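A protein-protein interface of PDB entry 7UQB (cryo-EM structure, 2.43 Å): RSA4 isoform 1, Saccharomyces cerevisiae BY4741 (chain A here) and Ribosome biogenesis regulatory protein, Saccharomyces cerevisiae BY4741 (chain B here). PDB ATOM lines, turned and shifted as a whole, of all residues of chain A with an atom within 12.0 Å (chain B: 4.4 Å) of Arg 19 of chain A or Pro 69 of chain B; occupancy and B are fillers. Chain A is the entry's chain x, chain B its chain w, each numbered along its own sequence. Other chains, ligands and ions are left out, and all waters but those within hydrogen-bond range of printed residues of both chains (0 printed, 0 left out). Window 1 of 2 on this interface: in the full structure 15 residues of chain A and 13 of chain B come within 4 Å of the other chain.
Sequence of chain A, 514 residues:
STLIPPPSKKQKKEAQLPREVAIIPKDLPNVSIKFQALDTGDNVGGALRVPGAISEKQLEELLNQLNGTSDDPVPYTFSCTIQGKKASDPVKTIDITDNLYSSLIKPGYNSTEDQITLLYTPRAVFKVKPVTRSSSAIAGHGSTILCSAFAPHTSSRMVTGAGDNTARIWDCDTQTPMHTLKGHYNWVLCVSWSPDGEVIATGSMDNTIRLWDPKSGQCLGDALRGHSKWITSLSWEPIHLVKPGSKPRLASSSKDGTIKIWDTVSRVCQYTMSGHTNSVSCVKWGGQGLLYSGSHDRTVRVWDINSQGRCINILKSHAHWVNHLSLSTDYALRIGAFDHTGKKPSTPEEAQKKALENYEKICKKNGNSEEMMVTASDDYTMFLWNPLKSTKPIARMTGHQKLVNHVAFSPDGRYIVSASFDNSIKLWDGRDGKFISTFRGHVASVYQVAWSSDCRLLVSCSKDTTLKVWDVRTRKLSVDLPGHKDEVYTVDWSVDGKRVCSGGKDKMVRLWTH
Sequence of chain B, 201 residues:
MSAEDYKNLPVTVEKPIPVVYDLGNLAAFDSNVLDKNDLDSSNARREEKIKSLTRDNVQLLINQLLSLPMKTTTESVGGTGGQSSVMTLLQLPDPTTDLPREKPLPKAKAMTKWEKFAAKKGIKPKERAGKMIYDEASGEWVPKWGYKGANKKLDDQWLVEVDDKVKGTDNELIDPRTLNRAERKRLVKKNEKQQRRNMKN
The side-chain amide nitrogen of Gln 64 of chain B is in hydrogen-bond range of the backbone carbonyl oxygen of Arg 19 of chain A (3.1 Å).
The backbone carbonyl oxygen of Pro 69 of chain B lies within hydrogen-bond range of the backbone NH of Gln 91 of chain B, at 2.9 Å.
Among the printed residues, merely in contact across the chains: Arg 19 of chain A with Ser 67 of chain B (3.7 Å), Arg 19 of chain A with Pro 69 of chain B (3.6 Å), Glu 20 of chain A with Ser 67 of chain B (3.7 Å) and Val 21 of chain A with Ser 67 of chain B (3.4 Å).
Lys 10 of chain A touches none of the printed residues of chain B.
Lys 13 of chain A touches none of the printed residues of chain B.
Arg 19 of chain A touches just these residues of chain B: Gln 64 (3.1 Å), Ser 67 (3.7 Å) and Pro 69 (3.6 Å).
Printed residues of chain B within 4 Å of Glu 20 of chain A: Ser 67.
Of the printed residues of chain B, Val 21 of chain A touches Ser 67 (3.4 Å).
Of chain A, only Arg 19 (3.1 Å) comes within 4 Å of Gln 64 of chain B.
Printed residues of chain A within 4 Å of Ser 67 of chain B: Arg 19 (3.7 Å), Glu 20 (3.7 Å) and Val 21 (3.4 Å).
No residue of chain A comes within 4 Å of Leu 68 of chain B.
Pro 69 of chain B touches just one residue of chain A: Arg 19.
No residue of chain A comes within 4 Å of Leu 90 of chain B.
No residue of chain A comes within 4 Å of Gln 91 of chain B.
The nearest residue of chain B that does not touch Arg 19 of chain A is Leu 68 of chain B (4.1 Å).
The nearest residue of chain A that does not touch Pro 69 of chain B is Ala 15 of chain A (6.5 Å).
The nearest printed residue of chain B that does not touch Glu 20 of chain A is Gln 64 of chain B (4.7 Å).
Hydrophobic or aromatic side chains of chain B that line the printed part of chain A: Pro 69.
Hydrophobic or aromatic side chains of chain A that line the printed part of chain B: Val 21.
Along chain A the printed residues that touch a printed residue of chain B span positions 19 to 21.
Among the printed residues, 5 pairs touch across the chains.
Among the printed residues, no Asp or Glu carboxylate lies within 4 Å of a Lys or Arg side-chain nitrogen of the other chain.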
ATOM      1  N   ILE A   4       5.481  -9.947  16.876  1.00  0.00           N
ATOM      2  CA  ILE A   4       5.117  -8.594  16.470  1.00  0.00           C
ATOM      3  C   ILE A   4       3.621  -8.595  16.171  1.00  0.00           C
ATOM      4  O   ILE A   4       3.070  -9.647  15.816  1.00  0.00           O
ATOM      5  CB  ILE A   4       5.952  -8.120  15.267  1.00  0.00           C
ATOM      6  CG1 ILE A   4       5.499  -8.796  13.974  1.00  0.00           C
ATOM      7  CG2 ILE A   4       7.428  -8.387  15.507  1.00  0.00           C
ATOM      8  CD1 ILE A   4       6.170  -8.249  12.735  1.00  0.00           C
ATOM      9  N   PRO A   7      -0.567  -7.469  10.837  1.00  0.00           N
ATOM     10  CA  PRO A   7      -1.175  -6.342  10.122  1.00  0.00           C
ATOM     11  C   PRO A   7      -2.693  -6.376  10.197  1.00  0.00           C
ATOM     12  O   PRO A   7      -3.316  -7.440  10.224  1.00  0.00           O
ATOM     13  CB  PRO A   7      -0.687  -6.532   8.682  1.00  0.00           C
ATOM     14  CG  PRO A   7      -0.411  -7.994   8.575  1.00  0.00           C
ATOM     15  CD  PRO A   7       0.121  -8.393   9.919  1.00  0.00           C
ATOM     16  N   LYS A  10      -7.077  -2.993   7.157  1.00  0.00           N
ATOM     17  CA  LYS A  10      -6.768  -1.861   6.287  1.00  0.00           C
ATOM     18  C   LYS A  10      -5.352  -1.958   5.734  1.00  0.00           C
ATOM     19  O   LYS A  10      -5.111  -1.623   4.567  1.00  0.00           O
ATOM     20  CB  LYS A  10      -6.959  -0.553   7.052  1.00  0.00           C
ATOM     21  CG  LYS A  10      -8.235  -0.506   7.874  1.00  0.00           C
ATOM     22  CD  LYS A  10      -8.406   0.842   8.556  1.00  0.00           C
ATOM     23  CE  LYS A  10      -9.646   0.856   9.436  1.00  0.00           C
ATOM     24  NZ  LYS A  10     -10.875   0.466   8.685  1.00  0.00           N
ATOM     25  N   GLN A  11      -4.403  -2.402   6.558  1.00  0.00           N
ATOM     26  CA  GLN A  11      -3.035  -2.583   6.085  1.00  0.00           C
ATOM     27  C   GLN A  11      -2.956  -3.679   5.030  1.00  0.00           C
ATOM     28  O   GLN A  11      -2.210  -3.551   4.053  1.00  0.00           O
ATOM     29  CB  GLN A  11      -2.111  -2.891   7.262  1.00  0.00           C
ATOM     30  CG  GLN A  11      -2.114  -1.816   8.334  1.00  0.00           C
ATOM     31  CD  GLN A  11      -1.165  -2.119   9.473  1.00  0.00           C
ATOM     32  OE1 GLN A  11      -1.520  -1.988  10.644  1.00  0.00           O
ATOM     33  NE2 GLN A  11       0.054  -2.522   9.135  1.00  0.00           N
ATOM     34  N   LYS A  12      -3.720  -4.761   5.204  1.00  0.00           N
ATOM     35  CA  LYS A  12      -3.754  -5.806   4.185  1.00  0.00           C
ATOM     36  C   LYS A  12      -4.362  -5.291   2.882  1.00  0.00           C
ATOM     37  O   LYS A  12      -3.894  -5.641   1.790  1.00  0.00           O
ATOM     38  CB  LYS A  12      -4.518  -7.023   4.709  1.00  0.00           C
ATOM     39  CG  LYS A  12      -3.828  -7.720   5.876  1.00  0.00           C
ATOM     40  CD  LYS A  12      -4.757  -8.688   6.591  1.00  0.00           C
ATOM     41  CE  LYS A  12      -4.723 -10.070   5.965  1.00  0.00           C
ATOM     42  NZ  LYS A  12      -3.436 -10.771   6.242  1.00  0.00           N
ATOM     43  N   LYS A  13      -5.397  -4.451   2.975  1.00  0.00           N
ATOM     44  CA  LYS A  13      -5.969  -3.836   1.777  1.00  0.00           C
ATOM     45  C   LYS A  13      -4.958  -2.935   1.070  1.00  0.00           C
ATOM     46  O   LYS A  13      -4.830  -2.972  -0.163  1.00  0.00           O
ATOM     47  CB  LYS A  13      -7.221  -3.041   2.145  1.00  0.00           C
ATOM     48  CG  LYS A  13      -8.384  -3.890   2.623  1.00  0.00           C
ATOM     49  CD  LYS A  13      -9.011  -4.657   1.477  1.00  0.00           C
ATOM     50  CE  LYS A  13      -9.523  -3.706   0.408  1.00  0.00           C
ATOM     51  NZ  LYS A  13     -10.564  -2.787   0.941  1.00  0.00           N
ATOM     52  N   GLU A  14      -4.230  -2.116   1.834  1.00  0.00           N
ATOM     53  CA  GLU A  14      -3.218  -1.253   1.231  1.00  0.00           C
ATOM     54  C   GLU A  14      -2.089  -2.070   0.615  1.00  0.00           C
ATOM     55  O   GLU A  14      -1.511  -1.675  -0.405  1.00  0.00           O
ATOM     56  CB  GLU A  14      -2.661  -0.273   2.265  1.00  0.00           C
ATOM     57  CG  GLU A  14      -3.413   1.042   2.347  1.00  0.00           C
ATOM     58  CD  GLU A  14      -2.709   2.064   3.221  1.00  0.00           C
ATOM     59  OE1 GLU A  14      -1.482   1.940   3.415  1.00  0.00           O
ATOM     60  OE2 GLU A  14      -3.385   2.990   3.716  1.00  0.00           O
ATOM     61  N   ALA A  15      -1.755  -3.209   1.224  1.00  0.00           N
ATOM     62  CA  ALA A  15      -0.751  -4.095   0.646  1.00  0.00           C
ATOM     63  C   ALA A  15      -1.243  -4.707  -0.658  1.00  0.00           C
ATOM     64  O   ALA A  15      -0.461  -4.897  -1.596  1.00  0.00           O
ATOM     65  CB  ALA A  15      -0.374  -5.186   1.648  1.00  0.00           C
ATOM     66  N   GLN A  16      -2.536  -5.034  -0.734  1.00  0.00           N
ATOM     67  CA  GLN A  16      -3.104  -5.533  -1.983  1.00  0.00           C
ATOM     68  C   GLN A  16      -3.202  -4.452  -3.051  1.00  0.00           C
ATOM     69  O   GLN A  16      -3.266  -4.782  -4.240  1.00  0.00           O
ATOM     70  CB  GLN A  16      -4.485  -6.134  -1.736  1.00  0.00           C
ATOM     71  CG  GLN A  16      -4.454  -7.526  -1.144  1.00  0.00           C
ATOM     72  CD  GLN A  16      -5.836  -8.038  -0.808  1.00  0.00           C
ATOM     73  OE1 GLN A  16      -6.731  -7.263  -0.472  1.00  0.00           O
ATOM     74  NE2 GLN A  16      -6.021  -9.348  -0.902  1.00  0.00           N
ATOM     75  N   LEU A  17      -3.235  -3.181  -2.656  1.00  0.00           N
ATOM     76  CA  LEU A  17      -3.225  -2.105  -3.638  1.00  0.00           C
ATOM     77  C   LEU A  17      -1.924  -2.132  -4.445  1.00  0.00           C
ATOM     78  O   LEU A  17      -0.870  -2.505  -3.922  1.00  0.00           O
ATOM     79  CB  LEU A  17      -3.381  -0.746  -2.956  1.00  0.00           C
ATOM     80  CG  LEU A  17      -4.758  -0.384  -2.405  1.00  0.00           C
ATOM     81  CD1 LEU A  17      -4.791   1.086  -2.020  1.00  0.00           C
ATOM     82  CD2 LEU A  17      -5.849  -0.702  -3.412  1.00  0.00           C
ATOM     83  N   PRO A  18      -1.975  -1.757  -5.728  1.00  0.00           N
ATOM     84  CA  PRO A  18      -0.769  -1.818  -6.566  1.00  0.00           C
ATOM     85  C   PRO A  18       0.333  -0.893  -6.070  1.00  0.00           C
ATOM     86  O   PRO A  18       0.078   0.196  -5.553  1.00  0.00           O
ATOM     87  CB  PRO A  18      -1.276  -1.389  -7.950  1.00  0.00           C
ATOM     88  CG  PRO A  18      -2.537  -0.639  -7.684  1.00  0.00           C
ATOM     89  CD  PRO A  18      -3.150  -1.307  -6.491  1.00  0.00           C
ATOM     90  N   ARG A  19       1.570  -1.345  -6.242  1.00  0.00           N
ATOM     91  CA  ARG A  19       2.743  -0.637  -5.758  1.00  0.00           C
ATOM     92  C   ARG A  19       3.277   0.317  -6.820  1.00  0.00           C
ATOM     93  O   ARG A  19       2.980   0.194  -8.010  1.00  0.00           O
ATOM     94  CB  ARG A  19       3.840  -1.626  -5.359  1.00  0.00           C
ATOM     95  CG  ARG A  19       3.381  -2.719  -4.410  1.00  0.00           C
ATOM     96  CD  ARG A  19       3.224  -2.188  -3.001  1.00  0.00           C
ATOM     97  NE  ARG A  19       4.484  -1.674  -2.481  1.00  0.00           N
ATOM     98  CZ  ARG A  19       4.683  -1.310  -1.222  1.00  0.00           C
ATOM     99  NH1 ARG A  19       3.721  -1.394  -0.319  1.00  0.00           N
ATOM    100  NH2 ARG A  19       5.879  -0.852  -0.860  1.00  0.00           N
ATOM    101  N   GLU A  20       4.079   1.275  -6.370  1.00  0.00           N
ATOM    102  CA  GLU A  20       4.747   2.211  -7.260  1.00  0.00           C
ATOM    103  C   GLU A  20       6.207   1.807  -7.420  1.00  0.00           C
ATOM    104  O   GLU A  20       6.871   1.431  -6.451  1.00  0.00           O
ATOM    105  CB  GLU A  20       4.636   3.647  -6.737  1.00  0.00           C
ATOM    106  CG  GLU A  20       5.126   3.864  -5.313  1.00  0.00           C
ATOM    107  CD  GLU A  20       6.567   4.333  -5.253  1.00  0.00           C
ATOM    108  OE1 GLU A  20       7.190   4.487  -6.324  1.00  0.00           O
ATOM    109  OE2 GLU A  20       7.076   4.556  -4.134  1.00  0.00           O
ATOM    110  N   VAL A  21       6.697   1.875  -8.655  1.00  0.00           N
ATOM    111  CA  VAL A  21       8.051   1.452  -8.994  1.00  0.00           C
ATOM    112  C   VAL A  21       8.946   2.681  -9.038  1.00  0.00           C
ATOM    113  O   VAL A  21       8.603   3.687  -9.672  1.00  0.00           O
ATOM    114  CB  VAL A  21       8.078   0.700 -10.335  1.00  0.00           C
ATOM    115  CG1 VAL A  21       9.470   0.160 -10.616  1.00  0.00           C
ATOM    116  CG2 VAL A  21       7.057  -0.424 -10.333  1.00  0.00           C
ATOM    117  N   ALA A  22      10.090   2.605  -8.362  1.00  0.00           N
ATOM    118  CA  ALA A  22      11.046   3.708  -8.328  1.00  0.00           C
ATOM    119  C   ALA A  22      11.947   3.609  -9.552  1.00  0.00           C
ATOM    120  O   ALA A  22      12.854   2.776  -9.608  1.00  0.00           O
ATOM    121  CB  ALA A  22      11.858   3.675  -7.038  1.00  0.00           C
ATOM    122  N   ILE A  23      11.704   4.470 -10.535  1.00  0.00           N
ATOM    123  CA  ILE A  23      12.440   4.469 -11.792  1.00  0.00           C
ATOM    124  C   ILE A  23      13.005   5.865 -12.020  1.00  0.00           C
ATOM    125  O   ILE A  23      12.385   6.867 -11.648  1.00  0.00           O
ATOM    126  CB  ILE A  23      11.547   4.018 -12.970  1.00  0.00           C
ATOM    127  CG1 ILE A  23      12.373   3.833 -14.243  1.00  0.00           C
ATOM    128  CG2 ILE A  23      10.389   4.986 -13.200  1.00  0.00           C
ATOM    129  CD1 ILE A  23      13.422   2.760 -14.125  1.00  0.00           C
ATOM    130  N   LYS A 106      15.610  12.088  -4.556  1.00  0.00           N
ATOM    131  CA  LYS A 106      14.348  11.409  -4.261  1.00  0.00           C
ATOM    132  C   LYS A 106      13.759  11.802  -2.908  1.00  0.00           C
ATOM    133  O   LYS A 106      12.548  12.077  -2.852  1.00  0.00           O
ATOM    134  CB  LYS A 106      14.532   9.892  -4.394  1.00  0.00           C
ATOM    135  CG  LYS A 106      13.290   9.079  -4.067  1.00  0.00           C
ATOM    136  CD  LYS A 106      13.555   7.590  -4.224  1.00  0.00           C
ATOM    137  CE  LYS A 106      12.288   6.777  -4.022  1.00  0.00           C
ATOM    138  NZ  LYS A 106      12.547   5.316  -4.134  1.00  0.00           N
ATOM    139  N   GLN B  64       6.741  -4.859 -10.189  1.00  0.00           N
ATOM    140  CA  GLN B  64       5.899  -4.802  -8.994  1.00  0.00           C
ATOM    141  C   GLN B  64       6.454  -5.675  -7.870  1.00  0.00           C
ATOM    142  O   GLN B  64       6.498  -5.252  -6.704  1.00  0.00           O
ATOM    143  CB  GLN B  64       4.470  -5.221  -9.343  1.00  0.00           C
ATOM    144  CG  GLN B  64       3.730  -4.232 -10.226  1.00  0.00           C
ATOM    145  CD  GLN B  64       3.344  -2.969  -9.484  1.00  0.00           C
ATOM    146  OE1 GLN B  64       3.289  -2.950  -8.255  1.00  0.00           O
ATOM    147  NE2 GLN B  64       3.071  -1.905 -10.227  1.00  0.00           N
ATOM    148  N   SER B  67       9.350  -4.129  -6.341  1.00  0.00           N
ATOM    149  CA  SER B  67       8.930  -2.964  -5.575  1.00  0.00           C
ATOM    150  C   SER B  67       8.193  -3.333  -4.295  1.00  0.00           C
ATOM    151  O   SER B  67       7.952  -2.451  -3.465  1.00  0.00           O
ATOM    152  CB  SER B  67       8.045  -2.062  -6.437  1.00  0.00           C
ATOM    153  OG  SER B  67       8.701  -1.718  -7.643  1.00  0.00           O
ATOM    154  N   LEU B  68       7.825  -4.603  -4.124  1.00  0.00           N
ATOM    155  CA  LEU B  68       7.185  -5.046  -2.892  1.00  0.00           C
ATOM    156  C   LEU B  68       8.124  -4.859  -1.697  1.00  0.00           C
ATOM    157  O   LEU B  68       9.349  -4.883  -1.850  1.00  0.00           O
ATOM    158  CB  LEU B  68       6.783  -6.516  -2.998  1.00  0.00           C
ATOM    159  CG  LEU B  68       5.415  -6.871  -3.581  1.00  0.00           C
ATOM    160  CD1 LEU B  68       5.275  -8.376  -3.703  1.00  0.00           C
ATOM    161  CD2 LEU B  68       4.308  -6.304  -2.714  1.00  0.00           C
ATOM    162  N   PRO B  69       7.576  -4.656  -0.499  1.00  0.00           N
ATOM    163  CA  PRO B  69       8.425  -4.586   0.696  1.00  0.00           C
ATOM    164  C   PRO B  69       9.115  -5.912   0.980  1.00  0.00           C
ATOM    165  O   PRO B  69       8.639  -6.990   0.610  1.00  0.00           O
ATOM    166  CB  PRO B  69       7.441  -4.217   1.814  1.00  0.00           C
ATOM    167  CG  PRO B  69       6.101  -4.604   1.292  1.00  0.00           C
ATOM    168  CD  PRO B  69       6.167  -4.370  -0.184  1.00  0.00           C
ATOM    169  N   MET B  70      10.268  -5.815   1.637  1.00  0.00           N
ATOM    170  CA  MET B  70      11.142  -6.956   1.853  1.00  0.00           C
ATOM    171  C   MET B  70      11.327  -7.221   3.340  1.00  0.00           C
ATOM    172  O   MET B  70      11.303  -6.303   4.165  1.00  0.00           O
ATOM    173  CB  MET B  70      12.505  -6.733   1.194  1.00  0.00           C
ATOM    174  CG  MET B  70      12.423  -6.434  -0.290  1.00  0.00           C
ATOM    175  SD  MET B  70      14.024  -6.039  -1.015  1.00  0.00           S
ATOM    176  CE  MET B  70      13.516  -5.455  -2.629  1.00  0.00           C
ATOM    177  N   LEU B  89      13.550 -11.731   1.676  1.00  0.00           N
ATOM    178  CA  LEU B  89      12.337 -12.335   1.142  1.00  0.00           C
ATOM    179  C   LEU B  89      11.299 -11.273   0.810  1.00  0.00           C
ATOM    180  O   LEU B  89      11.078 -10.345   1.587  1.00  0.00           O
ATOM    181  CB  LEU B  89      11.747 -13.340   2.133  1.00  0.00           C
ATOM    182  CG  LEU B  89      12.626 -14.551   2.442  1.00  0.00           C
ATOM    183  CD1 LEU B  89      11.916 -15.491   3.395  1.00  0.00           C
ATOM    184  CD2 LEU B  89      13.015 -15.273   1.163  1.00  0.00           C
ATOM    185  N   LEU B  90      10.656 -11.415  -0.345  1.00  0.00           N
ATOM    186  CA  LEU B  90       9.548 -10.536  -0.692  1.00  0.00           C
ATOM    187  C   LEU B  90       8.350 -10.819   0.204  1.00  0.00           C
ATOM    188  O   LEU B  90       8.054 -11.974   0.518  1.00  0.00           O
ATOM    189  CB  LEU B  90       9.154 -10.728  -2.154  1.00  0.00           C
ATOM    190  CG  LEU B  90      10.246 -10.497  -3.196  1.00  0.00           C
ATOM    191  CD1 LEU B  90       9.701 -10.756  -4.588  1.00  0.00           C
ATOM    192  CD2 LEU B  90      10.793  -9.088  -3.078  1.00  0.00           C
ATOM    193  N   GLN B  91       7.645  -9.763   0.612  1.00  0.00           N
ATOM    194  CA  GLN B  91       6.440  -9.911   1.421  1.00  0.00           C
ATOM    195  C   GLN B  91       5.234  -9.846   0.489  1.00  0.00           C
ATOM    196  O   GLN B  91       4.779  -8.763   0.116  1.00  0.00           O
ATOM    197  CB  GLN B  91       6.386  -8.845   2.510  1.00  0.00           C
ATOM    198  CG  GLN B  91       7.538  -8.958   3.499  1.00  0.00           C
ATOM    199  CD  GLN B  91       7.315  -8.163   4.764  1.00  0.00           C
ATOM    200  OE1 GLN B  91       7.760  -8.556   5.842  1.00  0.00           O
ATOM    201  NE2 GLN B  91       6.625  -7.037   4.644  1.00  0.00           N
